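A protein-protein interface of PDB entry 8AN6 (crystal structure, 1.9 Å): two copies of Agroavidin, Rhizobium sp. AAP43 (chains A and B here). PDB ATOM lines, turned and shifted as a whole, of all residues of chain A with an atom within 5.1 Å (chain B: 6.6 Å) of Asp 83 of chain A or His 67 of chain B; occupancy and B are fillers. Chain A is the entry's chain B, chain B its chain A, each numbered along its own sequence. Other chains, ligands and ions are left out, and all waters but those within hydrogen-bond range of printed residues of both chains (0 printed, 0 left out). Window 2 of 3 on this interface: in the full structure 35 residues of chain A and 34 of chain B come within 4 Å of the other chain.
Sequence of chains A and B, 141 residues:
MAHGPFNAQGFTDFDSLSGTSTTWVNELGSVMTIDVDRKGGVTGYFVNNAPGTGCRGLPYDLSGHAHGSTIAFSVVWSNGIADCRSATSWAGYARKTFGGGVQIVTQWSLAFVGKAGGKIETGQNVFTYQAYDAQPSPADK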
ATOM      1  N   CYS A  55     -30.224  -1.355  20.097  1.00  0.00           N
ATOM      2  CA  CYS A  55     -28.769  -1.220  19.893  1.00  0.00           C
ATOM      3  C   CYS A  55     -28.379  -1.837  18.551  1.00  0.00           C
ATOM      4  O   CYS A  55     -27.374  -2.548  18.502  1.00  0.00           O
ATOM      5  CB  CYS A  55     -28.016  -1.864  21.046  1.00  0.00           C
ATOM      6  SG  CYS A  55     -28.241  -0.957  22.594  1.00  0.00           S
ATOM      7  N   TYR A  60     -20.321  -3.033  18.643  1.00  0.00           N
ATOM      8  CA  TYR A  60     -20.027  -3.334  20.071  1.00  0.00           C
ATOM      9  C   TYR A  60     -18.782  -4.220  20.142  1.00  0.00           C
ATOM     10  O   TYR A  60     -18.686  -5.161  19.364  1.00  0.00           O
ATOM     11  CB  TYR A  60     -21.243  -3.950  20.765  1.00  0.00           C
ATOM     12  CG  TYR A  60     -22.366  -2.960  20.920  1.00  0.00           C
ATOM     13  CD1 TYR A  60     -22.366  -2.052  21.965  1.00  0.00           C
ATOM     14  CD2 TYR A  60     -23.377  -2.864  19.973  1.00  0.00           C
ATOM     15  CE1 TYR A  60     -23.369  -1.108  22.097  1.00  0.00           C
ATOM     16  CE2 TYR A  60     -24.373  -1.908  20.086  1.00  0.00           C
ATOM     17  CZ  TYR A  60     -24.353  -1.012  21.139  1.00  0.00           C
ATOM     18  OH  TYR A  60     -25.318  -0.058  21.261  1.00  0.00           O
ATOM     19  N   VAL A  76     -21.137  -6.856  25.714  1.00  0.00           N
ATOM     20  CA  VAL A  76     -22.071  -5.996  26.493  1.00  0.00           C
ATOM     21  C   VAL A  76     -22.614  -4.943  25.521  1.00  0.00           C
ATOM     22  O   VAL A  76     -21.829  -4.361  24.743  1.00  0.00           O
ATOM     23  CB  VAL A  76     -21.474  -5.403  27.788  1.00  0.00           C
ATOM     24  CG1 VAL A  76     -20.500  -4.259  27.555  1.00  0.00           C
ATOM     25  CG2 VAL A  76     -22.579  -4.930  28.720  1.00  0.00           C
ATOM     26  N   TRP A  77     -23.929  -4.733  25.543  1.00  0.00           N
ATOM     27  CA  TRP A  77     -24.630  -3.752  24.679  1.00  0.00           C
ATOM     28  C   TRP A  77     -24.465  -2.332  25.241  1.00  0.00           C
ATOM     29  O   TRP A  77     -25.476  -1.651  25.412  1.00  0.00           O
ATOM     30  CB  TRP A  77     -26.083  -4.188  24.505  1.00  0.00           C
ATOM     31  CG  TRP A  77     -26.137  -5.571  23.948  1.00  0.00           C
ATOM     32  CD1 TRP A  77     -26.443  -6.702  24.641  1.00  0.00           C
ATOM     33  CD2 TRP A  77     -25.755  -5.994  22.628  1.00  0.00           C
ATOM     34  NE1 TRP A  77     -26.331  -7.793  23.832  1.00  0.00           N
ATOM     35  CE2 TRP A  77     -25.897  -7.397  22.596  1.00  0.00           C
ATOM     36  CE3 TRP A  77     -25.295  -5.338  21.478  1.00  0.00           C
ATOM     37  CZ2 TRP A  77     -25.646  -8.149  21.453  1.00  0.00           C
ATOM     38  CZ3 TRP A  77     -25.048  -6.079  20.338  1.00  0.00           C
ATOM     39  CH2 TRP A  77     -25.211  -7.468  20.335  1.00  0.00           C
ATOM     40  N   SER A  78     -23.219  -1.887  25.444  1.00  0.00           N
ATOM     41  CA  SER A  78     -22.872  -0.491  25.836  1.00  0.00           C
ATOM     42  C   SER A  78     -21.546  -0.070  25.169  1.00  0.00           C
ATOM     43  O   SER A  78     -20.574  -0.825  25.277  1.00  0.00           O
ATOM     44  CB  SER A  78     -22.846  -0.350  27.340  1.00  0.00           C
ATOM     45  OG  SER A  78     -22.363   0.938  27.715  1.00  0.00           O
ATOM     46  N   ILE A  81     -22.348   5.125  23.177  1.00  0.00           N
ATOM     47  CA  ILE A  81     -23.282   5.670  22.155  1.00  0.00           C
ATOM     48  C   ILE A  81     -24.674   5.254  22.610  1.00  0.00           C
ATOM     49  O   ILE A  81     -25.376   6.108  23.180  1.00  0.00           O
ATOM     50  CB  ILE A  81     -22.956   5.185  20.723  1.00  0.00           C
ATOM     51  CG1 ILE A  81     -21.577   5.667  20.256  1.00  0.00           C
ATOM     52  CG2 ILE A  81     -24.063   5.597  19.756  1.00  0.00           C
ATOM     53  CD1 ILE A  81     -21.245   5.307  18.818  1.00  0.00           C
ATOM     54  N   ALA A  82     -25.026   3.984  22.398  1.00  0.00           N
ATOM     55  CA  ALA A  82     -26.317   3.391  22.815  1.00  0.00           C
ATOM     56  C   ALA A  82     -26.047   2.308  23.863  1.00  0.00           C
ATOM     57  O   ALA A  82     -25.070   1.539  23.712  1.00  0.00           O
ATOM     58  CB  ALA A  82     -27.070   2.862  21.623  1.00  0.00           C
ATOM     59  N   ASP A  83     -26.886   2.276  24.898  1.00  0.00           N
ATOM     60  CA  ASP A  83     -26.776   1.361  26.060  1.00  0.00           C
ATOM     61  C   ASP A  83     -28.122   0.662  26.206  1.00  0.00           C
ATOM     62  O   ASP A  83     -29.098   1.353  26.545  1.00  0.00           O
ATOM     63  CB  ASP A  83     -26.379   2.132  27.320  1.00  0.00           C
ATOM     64  CG  ASP A  83     -26.408   1.284  28.581  1.00  0.00           C
ATOM     65  OD1 ASP A  83     -26.481   0.026  28.455  1.00  0.00           O
ATOM     66  OD2 ASP A  83     -26.349   1.878  29.677  1.00  0.00           O
ATOM     67  N   CYS A  84     -28.188  -0.641  25.934  1.00  0.00           N
ATOM     68  CA  CYS A  84     -29.458  -1.417  25.971  1.00  0.00           C
ATOM     69  C   CYS A  84     -29.606  -2.132  27.319  1.00  0.00           C
ATOM     70  O   CYS A  84     -30.566  -2.921  27.446  1.00  0.00           O
ATOM     71  CB  CYS A  84     -29.578  -2.398  24.808  1.00  0.00           C
ATOM     72  SG  CYS A  84     -30.068  -1.634  23.244  1.00  0.00           S
ATOM     73  N   ARG A  85     -28.720  -1.866  28.287  1.00  0.00           N
ATOM     74  CA  ARG A  85     -28.779  -2.405  29.679  1.00  0.00           C
ATOM     75  C   ARG A  85     -28.856  -3.937  29.619  1.00  0.00           C
ATOM     76  O   ARG A  85     -29.721  -4.553  30.299  1.00  0.00           O
ATOM     77  CB  ARG A  85     -29.968  -1.843  30.469  1.00  0.00           C
ATOM     78  CG  ARG A  85     -29.726  -0.472  31.085  1.00  0.00           C
ATOM     79  CD  ARG A  85     -30.085   0.642  30.133  1.00  0.00           C
ATOM     80  NE  ARG A  85     -30.559   1.826  30.837  1.00  0.00           N
ATOM     81  CZ  ARG A  85     -30.855   2.988  30.259  1.00  0.00           C
ATOM     82  NH1 ARG A  85     -31.288   3.999  30.998  1.00  0.00           N
ATOM     83  NH2 ARG A  85     -30.718   3.136  28.949  1.00  0.00           N
ATOM     84  N   SER A  86     -27.971  -4.534  28.830  1.00  0.00           N
ATOM     85  CA  SER A  86     -28.031  -5.976  28.506  1.00  0.00           C
ATOM     86  C   SER A  86     -26.638  -6.456  28.119  1.00  0.00           C
ATOM     87  O   SER A  86     -25.720  -5.629  27.857  1.00  0.00           O
ATOM     88  CB  SER A  86     -29.067  -6.244  27.438  1.00  0.00           C
ATOM     89  OG  SER A  86     -28.752  -5.538  26.252  1.00  0.00           O
ATOM     90  N   ASP B  13     -23.760  -2.185  41.091  1.00  0.00           N
ATOM     91  CA  ASP B  13     -23.569  -2.740  39.701  1.00  0.00           C
ATOM     92  C   ASP B  13     -22.112  -2.575  39.219  1.00  0.00           C
ATOM     93  O   ASP B  13     -21.307  -1.951  39.937  1.00  0.00           O
ATOM     94  CB  ASP B  13     -24.577  -2.112  38.734  1.00  0.00           C
ATOM     95  CG  ASP B  13     -24.320  -0.653  38.390  1.00  0.00           C
ATOM     96  OD1 ASP B  13     -23.155  -0.179  38.540  1.00  0.00           O
ATOM     97  OD2 ASP B  13     -25.288  -0.006  37.954  1.00  0.00           O
ATOM     98  N   PHE B  14     -21.796  -3.071  38.012  1.00  0.00           N
ATOM     99  CA  PHE B  14     -20.407  -3.317  37.529  1.00  0.00           C
ATOM    100  C   PHE B  14     -19.720  -2.022  37.090  1.00  0.00           C
ATOM    101  O   PHE B  14     -18.525  -2.127  36.729  1.00  0.00           O
ATOM    102  CB  PHE B  14     -20.374  -4.333  36.380  1.00  0.00           C
ATOM    103  CG  PHE B  14     -21.146  -5.595  36.659  1.00  0.00           C
ATOM    104  CD1 PHE B  14     -20.739  -6.463  37.657  1.00  0.00           C
ATOM    105  CD2 PHE B  14     -22.288  -5.901  35.937  1.00  0.00           C
ATOM    106  CE1 PHE B  14     -21.473  -7.602  37.943  1.00  0.00           C
ATOM    107  CE2 PHE B  14     -23.017  -7.046  36.219  1.00  0.00           C
ATOM    108  CZ  PHE B  14     -22.606  -7.895  37.219  1.00  0.00           C
ATOM    109  N   ASP B  15     -20.413  -0.872  37.091  1.00  0.00           N
ATOM    110  CA  ASP B  15     -19.773   0.449  36.817  1.00  0.00           C
ATOM    111  C   ASP B  15     -18.818   0.793  37.970  1.00  0.00           C
ATOM    112  O   ASP B  15     -17.766   1.399  37.703  1.00  0.00           O
ATOM    113  CB  ASP B  15     -20.807   1.537  36.515  1.00  0.00           C
ATOM    114  CG  ASP B  15     -21.398   1.437  35.110  1.00  0.00           C
ATOM    115  OD1 ASP B  15     -20.909   0.588  34.313  1.00  0.00           O
ATOM    116  OD2 ASP B  15     -22.355   2.197  34.815  1.00  0.00           O
ATOM    117  N   LYS B  39     -13.057   0.906  30.354  1.00  0.00           N
ATOM    118  CA  LYS B  39     -13.977   0.748  29.195  1.00  0.00           C
ATOM    119  C   LYS B  39     -15.039  -0.337  29.457  1.00  0.00           C
ATOM    120  O   LYS B  39     -15.942  -0.478  28.610  1.00  0.00           O
ATOM    121  CB  LYS B  39     -13.149   0.388  27.958  1.00  0.00           C
ATOM    122  CG  LYS B  39     -13.773   0.770  26.629  1.00  0.00           C
ATOM    123  CD  LYS B  39     -12.828   0.575  25.463  1.00  0.00           C
ATOM    124  CE  LYS B  39     -13.439   0.995  24.140  1.00  0.00           C
ATOM    125  NZ  LYS B  39     -13.084   0.056  23.051  1.00  0.00           N
ATOM    126  N   GLY B  40     -14.933  -1.092  30.556  1.00  0.00           N
ATOM    127  CA  GLY B  40     -15.840  -2.216  30.870  1.00  0.00           C
ATOM    128  C   GLY B  40     -15.353  -3.548  30.304  1.00  0.00           C
ATOM    129  O   GLY B  40     -16.103  -4.550  30.391  1.00  0.00           O
ATOM    130  N   HIS B  65     -16.953  -8.571  29.014  1.00  0.00           N
ATOM    131  CA  HIS B  65     -17.367  -7.153  29.068  1.00  0.00           C
ATOM    132  C   HIS B  65     -18.357  -7.006  30.215  1.00  0.00           C
ATOM    133  O   HIS B  65     -19.089  -7.959  30.498  1.00  0.00           O
ATOM    134  CB  HIS B  65     -17.915  -6.716  27.704  1.00  0.00           C
ATOM    135  CG  HIS B  65     -16.847  -6.627  26.672  1.00  0.00           C
ATOM    136  ND1 HIS B  65     -15.950  -5.578  26.645  1.00  0.00           N
ATOM    137  CD2 HIS B  65     -16.492  -7.467  25.672  1.00  0.00           C
ATOM    138  CE1 HIS B  65     -15.088  -5.767  25.662  1.00  0.00           C
ATOM    139  NE2 HIS B  65     -15.419  -6.902  25.026  1.00  0.00           N
ATOM    140  N   ALA B  66     -18.316  -5.867  30.892  1.00  0.00           N
ATOM    141  CA  ALA B  66     -19.213  -5.552  32.012  1.00  0.00           C
ATOM    142  C   ALA B  66     -19.614  -4.089  31.876  1.00  0.00           C
ATOM    143  O   ALA B  66     -18.757  -3.274  31.536  1.00  0.00           O
ATOM    144  CB  ALA B  66     -18.521  -5.843  33.322  1.00  0.00           C
ATOM    145  N   HIS B  67     -20.896  -3.786  32.031  1.00  0.00           N
ATOM    146  CA  HIS B  67     -21.387  -2.387  32.072  1.00  0.00           C
ATOM    147  C   HIS B  67     -22.713  -2.362  32.809  1.00  0.00           C
ATOM    148  O   HIS B  67     -23.560  -3.240  32.539  1.00  0.00           O
ATOM    149  CB  HIS B  67     -21.495  -1.788  30.666  1.00  0.00           C
ATOM    150  CG  HIS B  67     -21.845  -0.340  30.678  1.00  0.00           C
ATOM    151  ND1 HIS B  67     -23.155   0.107  30.551  1.00  0.00           N
ATOM    152  CD2 HIS B  67     -21.066   0.761  30.821  1.00  0.00           C
ATOM    153  CE1 HIS B  67     -23.164   1.425  30.607  1.00  0.00           C
ATOM    154  NE2 HIS B  67     -21.890   1.849  30.772  1.00  0.00           N
ATOM    155  N   GLY B  68     -22.863  -1.383  33.700  1.00  0.00           N
ATOM    156  CA  GLY B  68     -24.095  -1.183  34.467  1.00  0.00           C
ATOM    157  C   GLY B  68     -24.393  -2.446  35.233  1.00  0.00           C
ATOM    158  O   GLY B  68     -23.483  -2.923  35.923  1.00  0.00           O
ATOM    159  N   SER B  69     -25.577  -3.013  35.025  1.00  0.00           N
ATOM    160  CA  SER B  69     -26.102  -4.167  35.795  1.00  0.00           C
ATOM    161  C   SER B  69     -25.911  -5.491  35.036  1.00  0.00           C
ATOM    162  O   SER B  69     -26.505  -6.495  35.477  1.00  0.00           O
ATOM    163  CB  SER B  69     -27.549  -3.949  36.105  1.00  0.00           C
ATOM    164  OG  SER B  69     -27.706  -2.905  37.040  1.00  0.00           O
ATOM    165  N   THR B  70     -25.163  -5.530  33.929  1.00  0.00           N
ATOM    166  CA  THR B  70     -25.005  -6.804  33.170  1.00  0.00           C
ATOM    167  C   THR B  70     -23.540  -7.052  32.814  1.00  0.00           C
ATOM    168  O   THR B  70     -22.747  -6.110  32.812  1.00  0.00           O
ATOM    169  CB  THR B  70     -25.942  -6.892  31.959  1.00  0.00           C
ATOM    170  OG1 THR B  70     -25.568  -5.973  30.931  1.00  0.00           O
ATOM    171  CG2 THR B  70     -27.389  -6.678  32.337  1.00  0.00           C
ATOM    172  N   ILE B  71     -23.243  -8.316  32.528  1.00  0.00           N
ATOM    173  CA  ILE B  71     -21.884  -8.848  32.256  1.00  0.00           C
ATOM    174  C   ILE B  71     -21.978 -10.101  31.363  1.00  0.00           C
ATOM    175  O   ILE B  71     -22.992 -10.859  31.416  1.00  0.00           O
ATOM    176  CB  ILE B  71     -21.151  -9.120  33.571  1.00  0.00           C
ATOM    177  CG1 ILE B  71     -19.715  -9.550  33.299  1.00  0.00           C
ATOM    178  CG2 ILE B  71     -21.881 -10.141  34.437  1.00  0.00           C
ATOM    179  CD1 ILE B  71     -18.840  -9.439  34.525  1.00  0.00           C
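Of the 11 printed residues of chain A, 5 touch a printed residue of chain B.
Hydrophobic or aromatic side chains of chain A that line the printed part of chain B: Val 76.
Along chain A the printed residues that touch a printed residue of chain B span positions 76 to 86.
Of the 12 printed residues of chain B, 3 touch a printed residue of chain A.
Among the printed residues, 7 pairs touch across the chains.
Among the printed residues, no Asp or Glu carboxylate lies within 4 Å of a Lys or Arg side-chain nitrogen of the other chain.
OG of Ser 86 of chain A lies within hydrogen-bond range of O of Cys 84 of chain A (3.4 Å).
The backbone NH of Trp 77 of chain A sits at hydrogen-bond distance from the backbone carbonyl oxygen of Ser 86 of chain A (3.1 Å).
SG of Cys 84 of chain A is disulfide-bonded to SG of Cys 55 of chain A.
N of Arg 85 of chain A lies within hydrogen-bond range of OD1 of Asp 83 of chain A.
A ring nitrogen (ND1) of His 67 of chain B lies close to the side-chain hydroxyl of Ser 78 of chain A (3.1 Å).
O of Ser 86 of chain A lies close to OG1 of Thr 70 of chain B, 3.1 Å away.
Printed residues of chain B within 4 Å of Ser 78 of chain A: His 67.
Of chain B, only His 67 (3.3 Å) comes within 4 Å of Asp 83 of chain A.
Of the printed residues of chain A, His 65 of chain B touches Val 76 (3.6 Å).
Of the printed residues of chain A, Thr 70 of chain B touches Val 76 (3.9 Å), Arg 85 (3.8 Å) and Ser 86 (3.0 Å).
Among the printed residues, merely in contact across the chains: Val 76 of chain A with His 65 of chain B, Val 76 of chain A with His 67 of chain B, Val 76 of chain A with Thr 70 of chain B, Asp 83 of chain A with His 67 of chain B and Arg 85 of chain A with Thr 70 of chain B.
No position is printed for both chains.
Of the 7 pairs that touch across the chains among the printed residues, none has its exchanged pair printed and touching as well.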
